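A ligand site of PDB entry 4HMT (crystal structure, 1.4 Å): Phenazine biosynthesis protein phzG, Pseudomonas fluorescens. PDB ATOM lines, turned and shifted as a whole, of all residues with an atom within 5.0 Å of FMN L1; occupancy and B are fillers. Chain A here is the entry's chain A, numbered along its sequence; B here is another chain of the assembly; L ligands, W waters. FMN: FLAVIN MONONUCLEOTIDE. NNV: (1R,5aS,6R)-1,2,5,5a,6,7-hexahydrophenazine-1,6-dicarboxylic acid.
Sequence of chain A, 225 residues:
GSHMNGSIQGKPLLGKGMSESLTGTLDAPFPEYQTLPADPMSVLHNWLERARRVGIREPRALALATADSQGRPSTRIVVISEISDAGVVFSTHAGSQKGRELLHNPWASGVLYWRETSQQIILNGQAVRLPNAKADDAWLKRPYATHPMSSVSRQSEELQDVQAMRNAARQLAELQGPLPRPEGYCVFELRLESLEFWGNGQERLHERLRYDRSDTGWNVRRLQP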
ATOM      1  N   GLU A  58     -15.555 -12.010  25.372  1.00  0.00           N
ATOM      2  CA  GLU A  58     -15.796 -10.719  26.043  1.00  0.00           C
ATOM      3  C   GLU A  58     -17.278 -10.462  26.304  1.00  0.00           C
ATOM      4  O   GLU A  58     -17.826  -9.444  25.911  1.00  0.00           O
ATOM      5  CB  GLU A  58     -15.079  -9.558  25.357  1.00  0.00           C
ATOM      6  CG  GLU A  58     -13.585  -9.662  25.371  1.00  0.00           C
ATOM      7  CD  GLU A  58     -12.900  -8.503  24.730  1.00  0.00           C
ATOM      8  OE1 GLU A  58     -13.320  -7.389  25.012  1.00  0.00           O
ATOM      9  OE2 GLU A  58     -11.967  -8.729  23.910  1.00  0.00           O
ATOM     10  N   ALA A  61     -18.340  -6.886  28.105  1.00  0.00           N
ATOM     11  CA  ALA A  61     -18.036  -5.609  27.404  1.00  0.00           C
ATOM     12  C   ALA A  61     -19.354  -4.872  27.203  1.00  0.00           C
ATOM     13  O   ALA A  61     -20.133  -5.238  26.356  1.00  0.00           O
ATOM     14  CB  ALA A  61     -17.336  -5.865  26.093  1.00  0.00           C
ATOM     15  N   THR A  75     -21.423   7.482  24.572  1.00  0.00           N
ATOM     16  CA  THR A  75     -21.229   6.027  24.723  1.00  0.00           C
ATOM     17  C   THR A  75     -19.777   5.646  24.706  1.00  0.00           C
ATOM     18  O   THR A  75     -18.912   6.402  24.203  1.00  0.00           O
ATOM     19  CB  THR A  75     -21.944   5.218  23.623  1.00  0.00           C
ATOM     20  OG1 THR A  75     -21.439   5.629  22.314  1.00  0.00           O
ATOM     21  CG2 THR A  75     -23.424   5.402  23.655  1.00  0.00           C
ATOM     22  N   ARG A  76     -19.477   4.475  25.288  1.00  0.00           N
ATOM     23  CA  ARG A  76     -18.155   3.858  25.307  1.00  0.00           C
ATOM     24  C   ARG A  76     -18.322   2.475  25.876  1.00  0.00           C
ATOM     25  O   ARG A  76     -19.292   2.197  26.551  1.00  0.00           O
ATOM     26  CB  ARG A  76     -17.128   4.664  26.129  1.00  0.00           C
ATOM     27  CG  ARG A  76     -17.309   4.499  27.640  1.00  0.00           C
ATOM     28  CD  ARG A  76     -18.568   5.139  28.140  1.00  0.00           C
ATOM     29  NE  ARG A  76     -18.546   6.557  27.960  1.00  0.00           N
ATOM     30  CZ  ARG A  76     -19.561   7.356  28.151  1.00  0.00           C
ATOM     31  NH1 ARG A  76     -19.367   8.664  28.090  1.00  0.00           N
ATOM     32  NH2 ARG A  76     -20.761   6.929  28.432  1.00  0.00           N
ATOM     33  N   ILE A  77     -17.334   1.615  25.635  1.00  0.00           N
ATOM     34  CA  ILE A  77     -17.322   0.308  26.287  1.00  0.00           C
ATOM     35  C   ILE A  77     -16.688   0.412  27.690  1.00  0.00           C
ATOM     36  O   ILE A  77     -15.667   1.088  27.889  1.00  0.00           O
ATOM     37  CB  ILE A  77     -16.496  -0.705  25.505  1.00  0.00           C
ATOM     38  CG1 ILE A  77     -17.024  -0.841  24.116  1.00  0.00           C
ATOM     39  CG2 ILE A  77     -16.514  -2.101  26.206  1.00  0.00           C
ATOM     40  CD1 ILE A  77     -18.482  -1.338  23.960  1.00  0.00           C
ATOM     41  N   VAL A  78     -17.323  -0.199  28.690  1.00  0.00           N
ATOM     42  CA  VAL A  78     -16.700  -0.450  29.994  1.00  0.00           C
ATOM     43  C   VAL A  78     -16.912  -1.935  30.282  1.00  0.00           C
ATOM     44  O   VAL A  78     -17.789  -2.585  29.703  1.00  0.00           O
ATOM     45  CB  VAL A  78     -17.294   0.376  31.133  1.00  0.00           C
ATOM     46  CG1 VAL A  78     -17.078   1.876  30.853  1.00  0.00           C
ATOM     47  CG2 VAL A  78     -18.803   0.086  31.427  1.00  0.00           C
ATOM     48  N   VAL A  79     -16.104  -2.471  31.191  1.00  0.00           N
ATOM     49  CA  VAL A  79     -16.268  -3.872  31.593  1.00  0.00           C
ATOM     50  C   VAL A  79     -17.046  -3.989  32.887  1.00  0.00           C
ATOM     51  O   VAL A  79     -16.727  -3.351  33.894  1.00  0.00           O
ATOM     52  CB  VAL A  79     -14.904  -4.565  31.788  1.00  0.00           C
ATOM     53  CG1 VAL A  79     -15.092  -6.009  32.196  1.00  0.00           C
ATOM     54  CG2 VAL A  79     -14.079  -4.487  30.541  1.00  0.00           C
ATOM     55  N   SER A  91     -15.680   0.059  37.055  1.00  0.00           N
ATOM     56  CA  SER A  91     -14.761   1.075  37.508  1.00  0.00           C
ATOM     57  C   SER A  91     -14.409   2.026  36.388  1.00  0.00           C
ATOM     58  O   SER A  91     -14.436   1.640  35.207  1.00  0.00           O
ATOM     59  CB  SER A  91     -13.441   0.418  37.975  1.00  0.00           C
ATOM     60  OG  SER A  91     -13.655  -0.360  39.131  1.00  0.00           O
ATOM     61  N   THR A  92     -14.052   3.253  36.742  1.00  0.00           N
ATOM     62  CA  THR A  92     -13.685   4.243  35.764  1.00  0.00           C
ATOM     63  C   THR A  92     -12.969   5.393  36.498  1.00  0.00           C
ATOM     64  O   THR A  92     -12.606   5.254  37.654  1.00  0.00           O
ATOM     65  CB  THR A  92     -14.901   4.757  34.987  1.00  0.00           C
ATOM     66  OG1 THR A  92     -14.453   5.453  33.821  1.00  0.00           O
ATOM     67  CG2 THR A  92     -15.783   5.590  35.733  1.00  0.00           C
ATOM     68  N   HIS A  93     -12.700   6.485  35.791  1.00  0.00           N
ATOM     69  CA  HIS A  93     -12.209   7.688  36.413  1.00  0.00           C
ATOM     70  C   HIS A  93     -13.270   8.744  36.540  1.00  0.00           C
ATOM     71  O   HIS A  93     -14.053   8.997  35.606  1.00  0.00           O
ATOM     72  CB  HIS A  93     -11.056   8.220  35.599  1.00  0.00           C
ATOM     73  CG  HIS A  93      -9.912   7.275  35.568  1.00  0.00           C
ATOM     74  ND1 HIS A  93      -8.802   7.416  36.382  1.00  0.00           N
ATOM     75  CD2 HIS A  93      -9.691   6.178  34.817  1.00  0.00           C
ATOM     76  CE1 HIS A  93      -7.968   6.423  36.138  1.00  0.00           C
ATOM     77  NE2 HIS A  93      -8.469   5.675  35.176  1.00  0.00           N
ATOM     78  N   SER A  96     -13.527  11.588  33.912  1.00  0.00           N
ATOM     79  CA  SER A  96     -13.792  11.233  32.510  1.00  0.00           C
ATOM     80  C   SER A  96     -15.126  11.815  32.096  1.00  0.00           C
ATOM     81  O   SER A  96     -15.851  12.397  32.907  1.00  0.00           O
ATOM     82  CB  SER A  96     -13.819   9.715  32.343  1.00  0.00           C
ATOM     83  OG  SER A  96     -14.926   9.161  33.045  1.00  0.00           O
ATOM     84  N   GLN A  97     -15.448  11.734  30.793  1.00  0.00           N
ATOM     85  CA  GLN A  97     -16.743  12.199  30.345  1.00  0.00           C
ATOM     86  C   GLN A  97     -17.894  11.476  31.051  1.00  0.00           C
ATOM     87  O   GLN A  97     -18.860  12.092  31.474  1.00  0.00           O
ATOM     88  CB  GLN A  97     -16.856  12.096  28.824  1.00  0.00           C
ATOM     89  CG  GLN A  97     -18.170  12.642  28.339  1.00  0.00           C
ATOM     90  CD  GLN A  97     -18.310  12.770  26.855  1.00  0.00           C
ATOM     91  OE1 GLN A  97     -17.413  12.469  26.112  1.00  0.00           O
ATOM     92  NE2 GLN A  97     -19.405  13.248  26.433  1.00  0.00           N
ATOM     93  N   LYS A  98     -17.791  10.145  31.125  1.00  0.00           N
ATOM     94  CA  LYS A  98     -18.844   9.383  31.744  1.00  0.00           C
ATOM     95  C   LYS A  98     -18.952   9.740  33.212  1.00  0.00           C
ATOM     96  O   LYS A  98     -20.053   9.803  33.733  1.00  0.00           O
ATOM     97  CB  LYS A  98     -18.679   7.861  31.506  1.00  0.00           C
ATOM     98  CG  LYS A  98     -17.785   7.146  32.516  1.00  0.00           C
ATOM     99  CD  LYS A  98     -17.388   5.763  32.109  1.00  0.00           C
ATOM    100  CE  LYS A  98     -16.354   5.765  30.999  1.00  0.00           C
ATOM    101  NZ  LYS A  98     -15.163   6.586  31.331  1.00  0.00           N
ATOM    102  N   GLY A  99     -17.832   9.965  33.903  1.00  0.00           N
ATOM    103  CA  GLY A  99     -17.901  10.283  35.312  1.00  0.00           C
ATOM    104  C   GLY A  99     -18.527  11.631  35.546  1.00  0.00           C
ATOM    105  O   GLY A  99     -19.340  11.783  36.449  1.00  0.00           O
ATOM    106  N   GLN A 155      -7.981  10.593  32.561  1.00  0.00           N
ATOM    107  CA  GLN A 155      -8.823  10.027  31.508  1.00  0.00           C
ATOM    108  C   GLN A 155      -9.737  11.044  30.846  1.00  0.00           C
ATOM    109  O   GLN A 155     -10.470  11.713  31.521  1.00  0.00           O
ATOM    110  CB  GLN A 155      -9.625   8.870  32.078  1.00  0.00           C
ATOM    111  CG  GLN A 155     -10.391   8.065  31.035  1.00  0.00           C
ATOM    112  CD  GLN A 155     -11.131   6.919  31.686  1.00  0.00           C
ATOM    113  OE1 GLN A 155     -12.068   7.136  32.446  1.00  0.00           O
ATOM    114  NE2 GLN A 155     -10.729   5.660  31.387  1.00  0.00           N
ATOM    115  N   SER A 156      -9.638  11.137  29.509  1.00  0.00           N
ATOM    116  CA  SER A 156     -10.497  11.929  28.622  1.00  0.00           C
ATOM    117  C   SER A 156     -10.152  13.406  28.545  1.00  0.00           C
ATOM    118  O   SER A 156     -10.735  14.132  27.743  1.00  0.00           O
ATOM    119  CB  SER A 156     -11.971  11.729  28.957  1.00  0.00           C
ATOM    120  OG  SER A 156     -12.273  10.353  29.050  1.00  0.00           O
ATOM    121  N   SER B  21      -9.347  -7.509  30.237  1.00  0.00           N
ATOM    122  CA  SER B  21     -10.373  -8.267  29.531  1.00  0.00           C
ATOM    123  C   SER B  21     -10.183  -8.266  28.029  1.00  0.00           C
ATOM    124  O   SER B  21     -10.839  -9.062  27.362  1.00  0.00           O
ATOM    125  CB  SER B  21     -11.754  -7.737  29.872  1.00  0.00           C
ATOM    126  OG  SER B  21     -11.973  -6.498  29.218  1.00  0.00           O
ATOM    127  N   LEU B  22      -9.263  -7.446  27.491  1.00  0.00           N
ATOM    128  CA  LEU B  22      -9.093  -7.410  26.035  1.00  0.00           C
ATOM    129  C   LEU B  22      -8.570  -8.725  25.507  1.00  0.00           C
ATOM    130  O   LEU B  22      -7.615  -9.277  26.083  1.00  0.00           O
ATOM    131  CB  LEU B  22      -8.131  -6.320  25.581  1.00  0.00           C
ATOM    132  CG  LEU B  22      -8.551  -4.921  25.978  1.00  0.00           C
ATOM    133  CD1 LEU B  22      -7.439  -3.946  25.569  1.00  0.00           C
ATOM    134  CD2 LEU B  22      -9.838  -4.507  25.320  1.00  0.00           C
ATOM    135  N   TYR B 113     -17.511  -1.719  18.578  1.00  0.00           N
ATOM    136  CA  TYR B 113     -16.406  -2.322  19.281  1.00  0.00           C
ATOM    137  C   TYR B 113     -16.056  -3.632  18.583  1.00  0.00           C
ATOM    138  O   TYR B 113     -16.936  -4.522  18.435  1.00  0.00           O
ATOM    139  CB  TYR B 113     -16.673  -2.540  20.741  1.00  0.00           C
ATOM    140  CG  TYR B 113     -15.585  -3.385  21.437  1.00  0.00           C
ATOM    141  CD1 TYR B 113     -14.242  -3.045  21.322  1.00  0.00           C
ATOM    142  CD2 TYR B 113     -15.906  -4.460  22.269  1.00  0.00           C
ATOM    143  CE1 TYR B 113     -13.262  -3.799  21.897  1.00  0.00           C
ATOM    144  CE2 TYR B 113     -14.877  -5.213  22.885  1.00  0.00           C
ATOM    145  CZ  TYR B 113     -13.586  -4.892  22.673  1.00  0.00           C
ATOM    146  OH  TYR B 113     -12.598  -5.634  23.272  1.00  0.00           O
ATOM    147  N   GLN B 120     -12.380   0.602  19.024  1.00  0.00           N
ATOM    148  CA  GLN B 120     -13.668   1.155  19.271  1.00  0.00           C
ATOM    149  C   GLN B 120     -13.836   2.400  18.404  1.00  0.00           C
ATOM    150  O   GLN B 120     -12.879   3.153  18.148  1.00  0.00           O
ATOM    151  CB  GLN B 120     -13.788   1.403  20.834  1.00  0.00           C
ATOM    152  CG  GLN B 120     -14.554   2.279  21.302  1.00  0.00           C
ATOM    153  CD  GLN B 120     -14.549   2.141  22.912  1.00  0.00           C
ATOM    154  OE1 GLN B 120     -15.567   2.012  23.424  1.00  0.00           O
ATOM    155  NE2 GLN B 120     -13.424   2.345  23.604  1.00  0.00           N
ATOM    156  N   GLU B 196     -14.868   9.547  17.953  1.00  0.00           N
ATOM    157  CA  GLU B 196     -13.623   9.089  18.531  1.00  0.00           C
ATOM    158  C   GLU B 196     -13.224   7.758  17.962  1.00  0.00           C
ATOM    159  O   GLU B 196     -14.049   6.857  17.851  1.00  0.00           O
ATOM    160  CB  GLU B 196     -13.679   9.000  20.044  1.00  0.00           C
ATOM    161  CG  GLU B 196     -12.360   8.499  20.662  1.00  0.00           C
ATOM    162  CD  GLU B 196     -12.385   8.275  22.195  1.00  0.00           C
ATOM    163  OE1 GLU B 196     -13.111   9.046  22.914  1.00  0.00           O
ATOM    164  OE2 GLU B 196     -11.649   7.342  22.646  1.00  0.00           O
ATOM    165  N   TRP B 198     -10.633   4.741  18.894  1.00  0.00           N
ATOM    166  CA  TRP B 198      -9.893   4.185  20.012  1.00  0.00           C
ATOM    167  C   TRP B 198      -9.163   2.935  19.564  1.00  0.00           C
ATOM    168  O   TRP B 198      -9.776   1.983  19.050  1.00  0.00           O
ATOM    169  CB  TRP B 198     -10.889   3.841  21.108  1.00  0.00           C
ATOM    170  CG  TRP B 198     -10.327   3.401  22.467  1.00  0.00           C
ATOM    171  CD1 TRP B 198     -10.299   4.167  23.578  1.00  0.00           C
ATOM    172  CD2 TRP B 198      -9.755   2.128  22.845  1.00  0.00           C
ATOM    173  NE1 TRP B 198      -9.779   3.490  24.635  1.00  0.00           N
ATOM    174  CE2 TRP B 198      -9.434   2.223  24.217  1.00  0.00           C
ATOM    175  CE3 TRP B 198      -9.536   0.906  22.178  1.00  0.00           C
ATOM    176  CZ2 TRP B 198      -8.868   1.180  24.909  1.00  0.00           C
ATOM    177  CZ3 TRP B 198      -8.957  -0.128  22.886  1.00  0.00           C
ATOM    178  CH2 TRP B 198      -8.644   0.015  24.244  1.00  0.00           C
ATOM    179  N   ARG B 208      -6.423   7.447  21.518  1.00  0.00           N
ATOM    180  CA  ARG B 208      -7.769   8.035  21.422  1.00  0.00           C
ATOM    181  C   ARG B 208      -7.642   9.275  20.559  1.00  0.00           C
ATOM    182  O   ARG B 208      -7.002  10.253  20.925  1.00  0.00           O
ATOM    183  CB  ARG B 208      -8.250   8.424  22.815  1.00  0.00           C
ATOM    184  CG  ARG B 208      -8.330   7.286  23.784  1.00  0.00           C
ATOM    185  CD  ARG B 208      -8.900   7.683  25.093  1.00  0.00           C
ATOM    186  NE  ARG B 208     -10.292   8.143  24.931  1.00  0.00           N
ATOM    187  CZ  ARG B 208     -11.021   8.691  25.895  1.00  0.00           C
ATOM    188  NH1 ARG B 208     -10.538   8.870  27.109  1.00  0.00           N
ATOM    189  NH2 ARG B 208     -12.300   9.007  25.680  1.00  0.00           N
ATOM    190  N   PRO B 225      -5.889   8.238  27.973  1.00  0.00           N
ATOM    191  CA  PRO B 225      -6.606   6.980  28.100  1.00  0.00           C
ATOM    192  C   PRO B 225      -7.318   6.727  29.386  1.00  0.00           C
ATOM    193  O   PRO B 225      -8.284   5.932  29.366  1.00  0.00           O
ATOM    194  CB  PRO B 225      -5.501   5.942  27.915  1.00  0.00           C
ATOM    195  CG  PRO B 225      -4.287   6.598  28.251  1.00  0.00           C
ATOM    196  CD  PRO B 225      -4.444   8.051  27.896  1.00  0.00           C
ATOM    197  OXT PRO B 225      -6.958   7.267  30.440  1.00  0.00           O
HETATM  198  N1  FMN L   1     -12.708   2.555  30.575  1.00  0.00           N
HETATM  199  C2  FMN L   1     -13.021   2.625  31.881  1.00  0.00           C
HETATM  200  O2  FMN L   1     -12.917   3.690  32.515  1.00  0.00           O
HETATM  201  N3  FMN L   1     -13.513   1.509  32.542  1.00  0.00           N
HETATM  202  C4  FMN L   1     -13.612   0.277  31.954  1.00  0.00           C
HETATM  203  O4  FMN L   1     -14.100  -0.669  32.573  1.00  0.00           O
HETATM  204  C4A FMN L   1     -13.249   0.204  30.616  1.00  0.00           C
HETATM  205  N5  FMN L   1     -13.318  -0.984  29.937  1.00  0.00           N
HETATM  206  C5A FMN L   1     -13.044  -0.993  28.603  1.00  0.00           C
HETATM  207  C6  FMN L   1     -13.211  -2.183  27.865  1.00  0.00           C
HETATM  208  C7  FMN L   1     -12.962  -2.297  26.504  1.00  0.00           C
HETATM  209  C7M FMN L   1     -13.185  -3.627  25.826  1.00  0.00           C
HETATM  210  C8  FMN L   1     -12.507  -1.164  25.813  1.00  0.00           C
HETATM  211  C8M FMN L   1     -12.192  -1.155  24.356  1.00  0.00           C
HETATM  212  C9  FMN L   1     -12.361   0.023  26.526  1.00  0.00           C
HETATM  213  C9A FMN L   1     -12.597   0.128  27.912  1.00  0.00           C
HETATM  214  N10 FMN L   1     -12.465   1.325  28.625  1.00  0.00           N
HETATM  215  C10 FMN L   1     -12.822   1.358  29.949  1.00  0.00           C
HETATM  216  C1' FMN L   1     -12.105   2.614  27.941  1.00  0.00           C
HETATM  217  C2' FMN L   1     -13.438   3.321  27.594  1.00  0.00           C
HETATM  218  O2' FMN L   1     -14.062   2.714  26.439  1.00  0.00           O
HETATM  219  C3' FMN L   1     -13.253   4.810  27.339  1.00  0.00           C
HETATM  220  O3' FMN L   1     -12.226   5.067  26.354  1.00  0.00           O
HETATM  221  C4' FMN L   1     -12.897   5.548  28.623  1.00  0.00           C
HETATM  222  O4' FMN L   1     -13.524   5.008  29.783  1.00  0.00           O
HETATM  223  C5' FMN L   1     -13.228   7.015  28.511  1.00  0.00           C
HETATM  224  O5' FMN L   1     -14.607   7.197  28.200  1.00  0.00           O
HETATM  225  P   FMN L   1     -15.294   8.620  28.299  1.00  0.00           P
HETATM  226  O1P FMN L   1     -15.655   8.854  29.775  1.00  0.00           O
HETATM  227  O2P FMN L   1     -14.327   9.631  27.735  1.00  0.00           O
HETATM  228  O3P FMN L   1     -16.528   8.521  27.429  1.00  0.00           O
HETATM  229  C01 NNV L   2      -9.355  -1.434  28.191  1.00  0.00           C
HETATM  230  C02 NNV L   2      -9.931  -2.633  28.766  1.00  0.00           C
HETATM  231  C03 NNV L   2     -10.334  -2.665  30.232  1.00  0.00           C
HETATM  232  C04 NNV L   2     -10.118  -1.380  30.953  1.00  0.00           C
HETATM  233  N05 NNV L   2     -10.586  -1.283  32.304  1.00  0.00           N
HETATM  234  C06 NNV L   2     -10.452  -0.053  33.015  1.00  0.00           C
HETATM  235  C07 NNV L   2     -10.913   0.006  34.401  1.00  0.00           C
HETATM  236  C08 NNV L   2     -10.863   1.295  35.059  1.00  0.00           C
HETATM  237  C09 NNV L   2     -10.335   2.482  34.423  1.00  0.00           C
HETATM  238  C10 NNV L   2      -9.794   1.042  32.427  1.00  0.00           C
HETATM  239  C11 NNV L   2      -9.513   2.283  33.208  1.00  0.00           C
HETATM  240  C12 NNV L   2      -7.991   2.339  33.552  1.00  0.00           C
HETATM  241  O13 NNV L   2      -7.466   3.440  33.992  1.00  0.00           O
HETATM  242  O14 NNV L   2      -7.172   1.361  33.381  1.00  0.00           O
HETATM  243  C15 NNV L   2      -9.618  -0.180  30.344  1.00  0.00           C
HETATM  244  C16 NNV L   2      -9.210  -0.169  28.905  1.00  0.00           C
HETATM  245  N17 NNV L   2      -9.510   0.947  31.077  1.00  0.00           N
HETATM  246  C18 NNV L   2      -9.731  -3.821  30.963  1.00  0.00           C
HETATM  247  O19 NNV L   2     -10.360  -4.919  30.800  1.00  0.00           O
HETATM  248  O20 NNV L   2      -8.642  -3.680  31.625  1.00  0.00           O
HETATM  249  O   HOH W   1     -14.805  -1.715  34.965  1.00  0.00           O
HETATM  250  O   HOH W   2     -13.539   5.958  24.288  1.00  0.00           O
HETATM  251  O   HOH W   3      -9.450   4.838  27.148  1.00  0.00           O
HETATM  252  O   HOH W   4     -14.802  11.640  25.935  1.00  0.00           O
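The side-chain hydroxyl (OG) of Ser 96 sits close to an oxygen (O1P) of FMN L1, 3.4 Å away.
The side-chain hydroxyl (OG) of Ser 156 lies within hydrogen-bond range of an oxygen (O2P) of FMN L1, 2.5 Å away.
The guanidinium group of Arg 76 is in salt-bridge range of an oxygen (O3P) of FMN L1, at 2.9 Å.
The backbone NH (N) of Val 79 sits at hydrogen-bond distance from an oxygen (O4) of FMN L1, 3.0 Å away.
The backbone NH (N) of Gln 97 is in hydrogen-bond range of an oxygen (O1P) of FMN L1 (3.1 Å).
O2' of FMN L1 is in hydrogen-bond range of O of Ile 77.
NE2 of His 93 is in hydrogen-bond range of O13 of NNV L2.
NH2 of Arg 208 of chain B lies within salt-bridge range of O2P of FMN L1, 3.0 Å away.
OG1 of Thr 92 sits at hydrogen-bond distance from O2 of FMN L1, 2.7 Å away.
A nitrogen (N3) of FMN L1 sits at hydrogen-bond distance from the backbone carbonyl oxygen (O) of Ser 91, 2.8 Å away.
An oxygen (O19) of NNV L2 lies within hydrogen-bond range of the backbone NH of Ser 21 of chain B, 2.8 Å away.
The indole nitrogen (NE1) of Trp 198 of chain B sits at hydrogen-bond distance from an oxygen (O3') of FMN L1 (3.4 Å).
An oxygen (O2') of FMN L1 sits at hydrogen-bond distance from the side-chain amide nitrogen (NE2) of Gln 120 of chain B, at 2.9 Å.
The side-chain amide nitrogen of Gln 155 sits at hydrogen-bond distance from an oxygen (O2) of FMN L1 (3.2 Å).
O1P of FMN L1 sits at hydrogen-bond distance from N of Lys 98, 2.8 Å away.
The side-chain amino group (NZ) of Lys 98 is in salt-bridge range of an oxygen (O1P) of FMN L1, 2.8 Å away.
The side-chain hydroxyl of Ser 21 of chain B is in hydrogen-bond range of an oxygen (O19) of NNV L2.
OG1 of Thr 92 is in hydrogen-bond range of NZ of Lys 98, 2.8 Å away.
The backbone carbonyl oxygen of His 93 sits at hydrogen-bond distance from the side-chain hydroxyl of Ser 96 (2.7 Å).
N of Trp 198 of chain B sits at hydrogen-bond distance from O of Gln 120 of chain B, 2.9 Å away.
The side-chain hydroxyl (OH) of Tyr 113 of chain B sits at hydrogen-bond distance from the side-chain carboxylate (OE1) of Glu 58 (2.6 Å).
The guanidinium group of Arg 208 of chain B sits at hydrogen-bond distance from the side-chain hydroxyl of Ser 156 (3.0 Å).
OG of Ser 96 lies within hydrogen-bond range of N of Gly 99 (3.1 Å).
O of Pro 225 of chain B is in hydrogen-bond range of NE2 of Gln 155 (3.2 Å).
The backbone NH (N) of His 93 is in hydrogen-bond range of the side-chain amide oxygen (OE1) of Gln 155 (3.5 Å).
OE1 of Glu 58 touches C7M of FMN L1, at 3.9 Å.
Val 78 touches FMN L1 (CA to N5, 3.4 Å).
CD2 of Leu 22 of chain B touches C7M of FMN L1, 3.5 Å away.
OH of Tyr 113 of chain B touches C7M of FMN L1 (3.3 Å).
Water W2 lies within hydrogen-bond range of O3' of FMN L1 (2.6 Å) and OE2 of Glu 196 of chain B (2.9 Å).
Water W1 lies within hydrogen-bond range of O4 of FMN L1 (2.7 Å), O of Val 79 (2.7 Å) and N of Ser 91 (2.9 Å).
Water W4 lies within hydrogen-bond range of an oxygen (O2P) of FMN L1 (2.7 Å) and the side-chain amide oxygen (OE1) of Gln 97 (2.7 Å).
Water W3 lies within hydrogen-bond range of the chain-end carboxylate of Pro 225 of chain B, the indole nitrogen of Trp 198 of chain B and an oxygen (O3') of FMN L1.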
